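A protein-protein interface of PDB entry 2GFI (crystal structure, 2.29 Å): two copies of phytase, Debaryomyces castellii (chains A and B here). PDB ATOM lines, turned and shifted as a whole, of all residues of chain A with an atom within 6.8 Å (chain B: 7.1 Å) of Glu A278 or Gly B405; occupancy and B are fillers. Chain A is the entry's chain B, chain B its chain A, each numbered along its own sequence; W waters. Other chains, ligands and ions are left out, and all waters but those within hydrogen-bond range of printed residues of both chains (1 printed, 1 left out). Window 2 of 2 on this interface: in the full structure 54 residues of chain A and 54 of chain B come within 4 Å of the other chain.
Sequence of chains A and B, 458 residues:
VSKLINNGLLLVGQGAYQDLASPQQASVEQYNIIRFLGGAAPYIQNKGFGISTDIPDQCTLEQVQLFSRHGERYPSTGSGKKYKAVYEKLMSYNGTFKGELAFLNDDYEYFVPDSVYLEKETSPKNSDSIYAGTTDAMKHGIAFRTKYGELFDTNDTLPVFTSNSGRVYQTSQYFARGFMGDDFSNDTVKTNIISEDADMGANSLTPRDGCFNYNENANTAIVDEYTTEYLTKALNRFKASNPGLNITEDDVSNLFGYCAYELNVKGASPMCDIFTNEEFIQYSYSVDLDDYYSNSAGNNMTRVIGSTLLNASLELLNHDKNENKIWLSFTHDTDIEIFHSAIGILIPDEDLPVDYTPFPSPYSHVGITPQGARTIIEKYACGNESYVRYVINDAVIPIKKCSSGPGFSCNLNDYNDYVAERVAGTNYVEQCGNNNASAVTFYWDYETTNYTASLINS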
ATOM      1  N   TYR A 226     -39.262  -6.453 -13.496  1.00  0.00           N
ATOM      2  CA  TYR A 226     -38.414  -6.036 -12.391  1.00  0.00           C
ATOM      3  C   TYR A 226     -37.531  -4.925 -12.906  1.00  0.00           C
ATOM      4  O   TYR A 226     -36.981  -5.027 -13.993  1.00  0.00           O
ATOM      5  CB  TYR A 226     -37.526  -7.195 -11.875  1.00  0.00           C
ATOM      6  CG  TYR A 226     -36.600  -6.772 -10.750  1.00  0.00           C
ATOM      7  CD1 TYR A 226     -37.113  -6.375  -9.523  1.00  0.00           C
ATOM      8  CD2 TYR A 226     -35.213  -6.748 -10.930  1.00  0.00           C
ATOM      9  CE1 TYR A 226     -36.273  -5.947  -8.498  1.00  0.00           C
ATOM     10  CE2 TYR A 226     -34.343  -6.345  -9.908  1.00  0.00           C
ATOM     11  CZ  TYR A 226     -34.894  -5.947  -8.688  1.00  0.00           C
ATOM     12  OH  TYR A 226     -34.076  -5.539  -7.674  1.00  0.00           O
ATOM     13  N   TYR A 230     -31.101   0.269 -12.299  1.00  0.00           N
ATOM     14  CA  TYR A 230     -29.740   0.260 -11.762  1.00  0.00           C
ATOM     15  C   TYR A 230     -28.744   0.049 -12.878  1.00  0.00           C
ATOM     16  O   TYR A 230     -27.637   0.533 -12.810  1.00  0.00           O
ATOM     17  CB  TYR A 230     -29.570  -0.801 -10.660  1.00  0.00           C
ATOM     18  CG  TYR A 230     -29.597  -2.218 -11.175  1.00  0.00           C
ATOM     19  CD1 TYR A 230     -28.411  -2.893 -11.399  1.00  0.00           C
ATOM     20  CD2 TYR A 230     -30.809  -2.865 -11.483  1.00  0.00           C
ATOM     21  CE1 TYR A 230     -28.399  -4.179 -11.892  1.00  0.00           C
ATOM     22  CE2 TYR A 230     -30.808  -4.172 -11.990  1.00  0.00           C
ATOM     23  CZ  TYR A 230     -29.582  -4.798 -12.197  1.00  0.00           C
ATOM     24  OH  TYR A 230     -29.487  -6.063 -12.704  1.00  0.00           O
ATOM     25  N   PHE A 275     -19.166  -2.135  -9.799  1.00  0.00           N
ATOM     26  CA  PHE A 275     -20.540  -2.044  -9.287  1.00  0.00           C
ATOM     27  C   PHE A 275     -20.601  -1.757  -7.798  1.00  0.00           C
ATOM     28  O   PHE A 275     -19.729  -2.164  -7.036  1.00  0.00           O
ATOM     29  CB  PHE A 275     -21.296  -3.351  -9.561  1.00  0.00           C
ATOM     30  CG  PHE A 275     -21.471  -3.645 -11.007  1.00  0.00           C
ATOM     31  CD1 PHE A 275     -22.201  -2.786 -11.814  1.00  0.00           C
ATOM     32  CD2 PHE A 275     -20.896  -4.762 -11.566  1.00  0.00           C
ATOM     33  CE1 PHE A 275     -22.370  -3.062 -13.162  1.00  0.00           C
ATOM     34  CE2 PHE A 275     -21.039  -5.047 -12.914  1.00  0.00           C
ATOM     35  CZ  PHE A 275     -21.780  -4.225 -13.708  1.00  0.00           C
ATOM     36  N   THR A 276     -21.666  -1.082  -7.395  1.00  0.00           N
ATOM     37  CA  THR A 276     -21.921  -0.841  -6.004  1.00  0.00           C
ATOM     38  C   THR A 276     -22.692  -2.029  -5.448  1.00  0.00           C
ATOM     39  O   THR A 276     -23.318  -2.796  -6.203  1.00  0.00           O
ATOM     40  CB  THR A 276     -22.803   0.405  -5.839  1.00  0.00           C
ATOM     41  OG1 THR A 276     -24.042   0.184  -6.519  1.00  0.00           O
ATOM     42  CG2 THR A 276     -22.182   1.662  -6.501  1.00  0.00           C
ATOM     43  N   ASN A 277     -22.689  -2.176  -4.127  1.00  0.00           N
ATOM     44  CA  ASN A 277     -23.451  -3.252  -3.504  1.00  0.00           C
ATOM     45  C   ASN A 277     -24.879  -3.241  -3.961  1.00  0.00           C
ATOM     46  O   ASN A 277     -25.502  -4.275  -4.148  1.00  0.00           O
ATOM     47  CB  ASN A 277     -23.425  -3.081  -1.996  1.00  0.00           C
ATOM     48  CG  ASN A 277     -22.107  -3.402  -1.433  1.00  0.00           C
ATOM     49  OD1 ASN A 277     -21.085  -3.205  -2.106  1.00  0.00           O
ATOM     50  ND2 ASN A 277     -22.090  -3.901  -0.208  1.00  0.00           N
ATOM     51  N   GLU A 278     -25.409  -2.041  -4.088  1.00  0.00           N
ATOM     52  CA  GLU A 278     -26.787  -1.857  -4.387  1.00  0.00           C
ATOM     53  C   GLU A 278     -27.126  -2.386  -5.802  1.00  0.00           C
ATOM     54  O   GLU A 278     -28.189  -2.946  -6.021  1.00  0.00           O
ATOM     55  CB  GLU A 278     -27.110  -0.382  -4.217  1.00  0.00           C
ATOM     56  CG  GLU A 278     -28.476  -0.022  -4.731  1.00  0.00           C
ATOM     57  CD  GLU A 278     -28.902   1.390  -4.357  1.00  0.00           C
ATOM     58  OE1 GLU A 278     -28.032   2.318  -4.180  1.00  0.00           O
ATOM     59  OE2 GLU A 278     -30.143   1.552  -4.250  1.00  0.00           O
ATOM     60  N   GLU A 279     -26.209  -2.218  -6.737  1.00  0.00           N
ATOM     61  CA  GLU A 279     -26.321  -2.783  -8.094  1.00  0.00           C
ATOM     62  C   GLU A 279     -26.225  -4.316  -8.036  1.00  0.00           C
ATOM     63  O   GLU A 279     -27.082  -5.009  -8.600  1.00  0.00           O
ATOM     64  CB  GLU A 279     -25.212  -2.180  -8.990  1.00  0.00           C
ATOM     65  CG  GLU A 279     -25.578  -0.739  -9.307  1.00  0.00           C
ATOM     66  CD  GLU A 279     -24.453   0.149  -9.702  1.00  0.00           C
ATOM     67  OE1 GLU A 279     -23.286  -0.226  -9.604  1.00  0.00           O
ATOM     68  OE2 GLU A 279     -24.747   1.292 -10.091  1.00  0.00           O
ATOM     69  N   PHE A 280     -25.204  -4.824  -7.324  1.00  0.00           N
ATOM     70  CA  PHE A 280     -25.093  -6.247  -7.057  1.00  0.00           C
ATOM     71  C   PHE A 280     -26.367  -6.830  -6.507  1.00  0.00           C
ATOM     72  O   PHE A 280     -26.818  -7.835  -7.019  1.00  0.00           O
ATOM     73  CB  PHE A 280     -23.971  -6.532  -6.089  1.00  0.00           C
ATOM     74  CG  PHE A 280     -22.625  -6.556  -6.735  1.00  0.00           C
ATOM     75  CD1 PHE A 280     -22.363  -7.432  -7.781  1.00  0.00           C
ATOM     76  CD2 PHE A 280     -21.625  -5.701  -6.299  1.00  0.00           C
ATOM     77  CE1 PHE A 280     -21.099  -7.484  -8.378  1.00  0.00           C
ATOM     78  CE2 PHE A 280     -20.354  -5.727  -6.908  1.00  0.00           C
ATOM     79  CZ  PHE A 280     -20.104  -6.628  -7.960  1.00  0.00           C
ATOM     80  N   ILE A 281     -26.967  -6.176  -5.503  1.00  0.00           N
ATOM     81  CA  ILE A 281     -28.178  -6.704  -4.871  1.00  0.00           C
ATOM     82  C   ILE A 281     -29.340  -6.780  -5.849  1.00  0.00           C
ATOM     83  O   ILE A 281     -30.155  -7.724  -5.822  1.00  0.00           O
ATOM     84  CB  ILE A 281     -28.536  -5.894  -3.609  1.00  0.00           C
ATOM     85  CG1 ILE A 281     -27.528  -6.228  -2.482  1.00  0.00           C
ATOM     86  CG2 ILE A 281     -29.960  -6.192  -3.148  1.00  0.00           C
ATOM     87  CD1 ILE A 281     -27.530  -5.231  -1.391  1.00  0.00           C
ATOM     88  N   GLN A 282     -29.418  -5.801  -6.730  1.00  0.00           N
ATOM     89  CA  GLN A 282     -30.524  -5.777  -7.686  1.00  0.00           C
ATOM     90  C   GLN A 282     -30.261  -6.733  -8.802  1.00  0.00           C
ATOM     91  O   GLN A 282     -31.178  -7.424  -9.238  1.00  0.00           O
ATOM     92  CB  GLN A 282     -30.785  -4.371  -8.222  1.00  0.00           C
ATOM     93  CG  GLN A 282     -31.408  -3.469  -7.192  1.00  0.00           C
ATOM     94  CD  GLN A 282     -31.287  -2.044  -7.610  1.00  0.00           C
ATOM     95  OE1 GLN A 282     -32.260  -1.471  -8.108  1.00  0.00           O
ATOM     96  NE2 GLN A 282     -30.068  -1.473  -7.496  1.00  0.00           N
ATOM     97  N   TYR A 283     -29.010  -6.807  -9.249  1.00  0.00           N
ATOM     98  CA  TYR A 283     -28.679  -7.862 -10.191  1.00  0.00           C
ATOM     99  C   TYR A 283     -29.053  -9.242  -9.632  1.00  0.00           C
ATOM    100  O   TYR A 283     -29.673 -10.092 -10.325  1.00  0.00           O
ATOM    101  CB  TYR A 283     -27.218  -7.853 -10.547  1.00  0.00           C
ATOM    102  CG  TYR A 283     -26.861  -9.039 -11.426  1.00  0.00           C
ATOM    103  CD1 TYR A 283     -27.158  -9.038 -12.812  1.00  0.00           C
ATOM    104  CD2 TYR A 283     -26.254 -10.176 -10.875  1.00  0.00           C
ATOM    105  CE1 TYR A 283     -26.832 -10.141 -13.623  1.00  0.00           C
ATOM    106  CE2 TYR A 283     -25.927 -11.268 -11.656  1.00  0.00           C
ATOM    107  CZ  TYR A 283     -26.219 -11.249 -13.019  1.00  0.00           C
ATOM    108  OH  TYR A 283     -25.862 -12.326 -13.763  1.00  0.00           O
ATOM    109  N   GLY B  50     -26.338  -7.087   2.972  1.00  0.00           N
ATOM    110  CA  GLY B  50     -25.220  -6.765   2.108  1.00  0.00           C
ATOM    111  C   GLY B  50     -25.262  -5.344   1.613  1.00  0.00           C
ATOM    112  O   GLY B  50     -24.428  -4.961   0.821  1.00  0.00           O
ATOM    113  N   ILE B  51     -26.235  -4.560   2.094  1.00  0.00           N
ATOM    114  CA  ILE B  51     -26.404  -3.177   1.699  1.00  0.00           C
ATOM    115  C   ILE B  51     -25.333  -2.382   2.347  1.00  0.00           C
ATOM    116  O   ILE B  51     -25.083  -2.500   3.559  1.00  0.00           O
ATOM    117  CB  ILE B  51     -27.787  -2.648   2.083  1.00  0.00           C
ATOM    118  CG1 ILE B  51     -28.873  -3.490   1.396  1.00  0.00           C
ATOM    119  CG2 ILE B  51     -27.936  -1.237   1.633  1.00  0.00           C
ATOM    120  CD1 ILE B  51     -30.188  -3.359   2.043  1.00  0.00           C
ATOM    121  N   SER B  52     -24.649  -1.588   1.549  1.00  0.00           N
ATOM    122  CA  SER B  52     -23.591  -0.783   2.120  1.00  0.00           C
ATOM    123  C   SER B  52     -24.216   0.240   3.090  1.00  0.00           C
ATOM    124  O   SER B  52     -25.277   0.843   2.818  1.00  0.00           O
ATOM    125  CB  SER B  52     -22.760  -0.187   1.005  1.00  0.00           C
ATOM    126  OG  SER B  52     -22.176   1.018   1.455  1.00  0.00           O
ATOM    127  N   PRO B  56     -24.900   6.733   0.378  1.00  0.00           N
ATOM    128  CA  PRO B  56     -24.629   6.532  -1.021  1.00  0.00           C
ATOM    129  C   PRO B  56     -23.925   7.743  -1.615  1.00  0.00           C
ATOM    130  O   PRO B  56     -24.200   8.869  -1.223  1.00  0.00           O
ATOM    131  CB  PRO B  56     -26.037   6.363  -1.619  1.00  0.00           C
ATOM    132  CG  PRO B  56     -26.832   5.870  -0.480  1.00  0.00           C
ATOM    133  CD  PRO B  56     -26.339   6.619   0.666  1.00  0.00           C
ATOM    134  N   TYR B 380     -31.159  11.446   3.992  1.00  0.00           N
ATOM    135  CA  TYR B 380     -30.189  12.095   3.140  1.00  0.00           C
ATOM    136  C   TYR B 380     -30.806  12.536   1.830  1.00  0.00           C
ATOM    137  O   TYR B 380     -31.812  11.980   1.363  1.00  0.00           O
ATOM    138  CB  TYR B 380     -28.966  11.184   2.866  1.00  0.00           C
ATOM    139  CG  TYR B 380     -29.283   9.750   2.457  1.00  0.00           C
ATOM    140  CD1 TYR B 380     -29.825   9.453   1.197  1.00  0.00           C
ATOM    141  CD2 TYR B 380     -29.017   8.695   3.338  1.00  0.00           C
ATOM    142  CE1 TYR B 380     -30.122   8.135   0.840  1.00  0.00           C
ATOM    143  CE2 TYR B 380     -29.262   7.391   2.998  1.00  0.00           C
ATOM    144  CZ  TYR B 380     -29.815   7.098   1.751  1.00  0.00           C
ATOM    145  OH  TYR B 380     -30.055   5.781   1.427  1.00  0.00           O
ATOM    146  N   CYS B 382     -30.661  13.195  -2.153  1.00  0.00           N
ATOM    147  CA  CYS B 382     -30.043  12.777  -3.386  1.00  0.00           C
ATOM    148  C   CYS B 382     -30.765  13.577  -4.444  1.00  0.00           C
ATOM    149  O   CYS B 382     -31.975  13.390  -4.641  1.00  0.00           O
ATOM    150  CB  CYS B 382     -30.249  11.284  -3.606  1.00  0.00           C
ATOM    151  SG  CYS B 382     -29.634  10.771  -5.216  1.00  0.00           S
ATOM    152  N   TYR B 387     -34.396  11.191   1.206  1.00  0.00           N
ATOM    153  CA  TYR B 387     -34.596   9.765   1.421  1.00  0.00           C
ATOM    154  C   TYR B 387     -34.354   9.415   2.875  1.00  0.00           C
ATOM    155  O   TYR B 387     -33.541  10.033   3.560  1.00  0.00           O
ATOM    156  CB  TYR B 387     -33.688   8.962   0.508  1.00  0.00           C
ATOM    157  CG  TYR B 387     -34.039   9.200  -0.928  1.00  0.00           C
ATOM    158  CD1 TYR B 387     -35.004   8.426  -1.563  1.00  0.00           C
ATOM    159  CD2 TYR B 387     -33.435  10.238  -1.643  1.00  0.00           C
ATOM    160  CE1 TYR B 387     -35.347   8.672  -2.879  1.00  0.00           C
ATOM    161  CE2 TYR B 387     -33.756  10.484  -2.947  1.00  0.00           C
ATOM    162  CZ  TYR B 387     -34.716   9.716  -3.559  1.00  0.00           C
ATOM    163  OH  TYR B 387     -35.042   9.971  -4.862  1.00  0.00           O
ATOM    164  N   ARG B 389     -33.887   5.925   5.507  1.00  0.00           N
ATOM    165  CA  ARG B 389     -33.772   4.480   5.636  1.00  0.00           C
ATOM    166  C   ARG B 389     -33.381   4.108   7.054  1.00  0.00           C
ATOM    167  O   ARG B 389     -32.878   4.939   7.815  1.00  0.00           O
ATOM    168  CB  ARG B 389     -32.777   3.893   4.616  1.00  0.00           C
ATOM    169  CG  ARG B 389     -31.341   4.190   4.928  1.00  0.00           C
ATOM    170  CD  ARG B 389     -30.389   3.474   4.013  1.00  0.00           C
ATOM    171  NE  ARG B 389     -29.030   3.869   4.301  1.00  0.00           N
ATOM    172  CZ  ARG B 389     -27.992   3.500   3.572  1.00  0.00           C
ATOM    173  NH1 ARG B 389     -28.191   2.736   2.487  1.00  0.00           N
ATOM    174  NH2 ARG B 389     -26.763   3.911   3.906  1.00  0.00           N
ATOM    175  N   CYS B 402     -40.859   0.254  -0.007  1.00  0.00           N
ATOM    176  CA  CYS B 402     -40.315   1.607  -0.023  1.00  0.00           C
ATOM    177  C   CYS B 402     -38.812   1.619   0.027  1.00  0.00           C
ATOM    178  O   CYS B 402     -38.223   2.128   0.967  1.00  0.00           O
ATOM    179  CB  CYS B 402     -40.810   2.475   1.103  1.00  0.00           C
ATOM    180  SG  CYS B 402     -40.846   4.162   0.467  1.00  0.00           S
ATOM    181  N   SER B 403     -38.192   1.070  -0.996  1.00  0.00           N
ATOM    182  CA  SER B 403     -36.774   0.881  -0.962  1.00  0.00           C
ATOM    183  C   SER B 403     -36.167   1.123  -2.334  1.00  0.00           C
ATOM    184  O   SER B 403     -35.099   0.592  -2.657  1.00  0.00           O
ATOM    185  CB  SER B 403     -36.481  -0.530  -0.471  1.00  0.00           C
ATOM    186  OG  SER B 403     -37.277  -1.453  -1.172  1.00  0.00           O
ATOM    187  N   SER B 404     -36.839   1.925  -3.157  1.00  0.00           N
ATOM    188  CA  SER B 404     -36.290   2.188  -4.485  1.00  0.00           C
ATOM    189  C   SER B 404     -35.404   3.445  -4.532  1.00  0.00           C
ATOM    190  O   SER B 404     -34.783   3.723  -5.555  1.00  0.00           O
ATOM    191  CB  SER B 404     -37.389   2.216  -5.551  1.00  0.00           C
ATOM    192  OG  SER B 404     -38.394   3.105  -5.156  1.00  0.00           O
ATOM    193  N   GLY B 405     -35.302   4.179  -3.420  1.00  0.00           N
ATOM    194  CA  GLY B 405     -34.367   5.304  -3.370  1.00  0.00           C
ATOM    195  C   GLY B 405     -32.945   4.785  -3.320  1.00  0.00           C
ATOM    196  O   GLY B 405     -32.743   3.581  -3.188  1.00  0.00           O
ATOM    197  N   PRO B 406     -31.948   5.667  -3.416  1.00  0.00           N
ATOM    198  CA  PRO B 406     -30.541   5.247  -3.298  1.00  0.00           C
ATOM    199  C   PRO B 406     -30.261   4.585  -1.938  1.00  0.00           C
ATOM    200  O   PRO B 406     -30.823   5.007  -0.930  1.00  0.00           O
ATOM    201  CB  PRO B 406     -29.766   6.567  -3.404  1.00  0.00           C
ATOM    202  CG  PRO B 406     -30.724   7.504  -4.082  1.00  0.00           C
ATOM    203  CD  PRO B 406     -32.085   7.126  -3.601  1.00  0.00           C
ATOM    204  N   GLY B 407     -29.432   3.544  -1.922  1.00  0.00           N
ATOM    205  CA  GLY B 407     -29.147   2.782  -0.702  1.00  0.00           C
ATOM    206  C   GLY B 407     -30.393   2.072  -0.184  1.00  0.00           C
ATOM    207  O   GLY B 407     -30.510   1.847   1.016  1.00  0.00           O
ATOM    208  N   PHE B 408     -31.318   1.741  -1.092  1.00  0.00           N
ATOM    209  CA  PHE B 408     -32.621   1.119  -0.771  1.00  0.00           C
ATOM    210  C   PHE B 408     -33.463   1.882   0.240  1.00  0.00           C
ATOM    211  O   PHE B 408     -34.127   1.303   1.120  1.00  0.00           O
ATOM    212  CB  PHE B 408     -32.466  -0.353  -0.379  1.00  0.00           C
ATOM    213  CG  PHE B 408     -31.858  -1.174  -1.455  1.00  0.00           C
ATOM    214  CD1 PHE B 408     -32.615  -1.549  -2.574  1.00  0.00           C
ATOM    215  CD2 PHE B 408     -30.532  -1.576  -1.366  1.00  0.00           C
ATOM    216  CE1 PHE B 408     -32.033  -2.316  -3.604  1.00  0.00           C
ATOM    217  CE2 PHE B 408     -29.940  -2.355  -2.364  1.00  0.00           C
ATOM    218  CZ  PHE B 408     -30.694  -2.714  -3.491  1.00  0.00           C
ATOM    219  N   SER B 409     -33.441   3.207   0.064  1.00  0.00           N
ATOM    220  CA  SER B 409     -34.099   4.134   0.950  1.00  0.00           C
ATOM    221  C   SER B 409     -35.504   4.485   0.455  1.00  0.00           C
ATOM    222  O   SER B 409     -35.904   4.152  -0.660  1.00  0.00           O
ATOM    223  CB  SER B 409     -33.243   5.392   1.057  1.00  0.00           C
ATOM    224  OG  SER B 409     -33.024   5.943  -0.237  1.00  0.00           O
ATOM    225  N   CYS B 410     -36.244   5.170   1.306  1.00  0.00           N
ATOM    226  CA  CYS B 410     -37.605   5.558   1.037  1.00  0.00           C
ATOM    227  C   CYS B 410     -37.686   7.087   0.876  1.00  0.00           C
ATOM    228  O   CYS B 410     -37.259   7.814   1.791  1.00  0.00           O
ATOM    229  CB  CYS B 410     -38.445   5.149   2.223  1.00  0.00           C
ATOM    230  SG  CYS B 410     -40.182   5.355   1.933  1.00  0.00           S
ATOM    231  N   ASN B 411     -38.210   7.568  -0.263  1.00  0.00           N
ATOM    232  CA  ASN B 411     -38.441   9.007  -0.434  1.00  0.00           C
ATOM    233  C   ASN B 411     -39.243   9.501   0.756  1.00  0.00           C
ATOM    234  O   ASN B 411     -40.233   8.887   1.142  1.00  0.00           O
ATOM    235  CB  ASN B 411     -39.221   9.299  -1.728  1.00  0.00           C
ATOM    236  CG  ASN B 411     -39.147  10.767  -2.150  1.00  0.00           C
ATOM    237  OD1 ASN B 411     -39.526  11.670  -1.404  1.00  0.00           O
ATOM    238  ND2 ASN B 411     -38.663  11.005  -3.364  1.00  0.00           N
HETATM  239  O   HOH W   1     -25.699  -0.681  -0.985  1.00  0.00           O
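The backbone NH (N) of Gly B407 sits at hydrogen-bond distance from the side-chain carboxylate (OE1) of Glu A278 (2.9 Å). The side-chain amide nitrogen (ND2) of Asn A277 sits at hydrogen-bond distance from the backbone carbonyl oxygen (O) of Gly B50, 2.8 Å away. The backbone NH of Phe B408 sits at hydrogen-bond distance from the side-chain carboxylate of Glu A278. OE2 of Glu A278 lies close to O of Gly B405, at 3.5 Å.
The side-chain hydroxyl (OG) of Ser B409 lies within hydrogen-bond range of the backbone carbonyl oxygen (O) of Pro B406 (2.5 Å). NE2 of Gln A282 sits at hydrogen-bond distance from O of Glu A278 (2.8 Å). The guanidinium group (NH1) of Arg B389 lies within hydrogen-bond range of the backbone carbonyl oxygen (O) of Gly B407 (2.9 Å). The backbone carbonyl oxygen of Ser B52 lies within hydrogen-bond range of the guanidinium group of Arg B389, 3.5 Å away. The backbone carbonyl oxygen (O) of Pro B406 sits at hydrogen-bond distance from the side-chain hydroxyl (OH) of Tyr B380 (2.6 Å). The side-chain sulfur of Cys B410 is disulfide-bonded to the side-chain sulfur of Cys B402 (2.0 Å).
Asn A277 touches Ser B52 (ND2 to N, 3.9 Å). Glu A278 touches Pro B406 (OE2 to C, 3.8 Å). CD1 of Ile A281 touches C of Gly B50, at 3.8 Å. CD1 of Ile A281 touches CG1 of Ile B51 (3.5 Å). CG2 of Ile A281 touches CZ of Phe B408, at 3.6 Å. Phe B408 touches Gln A282 (CE1 to CG, 3.8 Å).
Glu A278 touches four residues of chain B. Of the printed residues of chain B, Ile A281 touches Gly B50, Ile B51 and Phe B408. Printed residues of chain B within 4 Å of Gln A282: Phe B408 (3.8 Å). Gly B405 touches just one residue of chain A: Glu A278. Printed residues of chain A within 4 Å of Pro B406: Glu A278 (3.8 Å). Of the printed residues of chain A, Gly B407 touches Glu A278. Of the printed residues of chain A, Phe B408 touches Glu A278, Ile A281 and Gln A282. The nearest printed residue of chain A that does not touch Gly B405 is Gln A282 (7.1 Å).
Of the 11 printed residues of chain A, 4 touch a printed residue of chain B. Hydrophobic or aromatic side chains of chain A within 4 Å of the printed part of chain B: Ile A281. Hydrophobic or aromatic side chains of chain B that line the printed part of chain A: Ile B51 and Phe B408. Among the printed residues, 10 pairs touch across the chains.
No position is printed for both chains. Of the 10 pairs that touch across the chains among the printed residues, none has its exchanged pair printed and touching as well.
Water W1 bridges the backbone NH of Ser B52 (2.9 Å) and the backbone NH of Glu A278 (3.4 Å).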
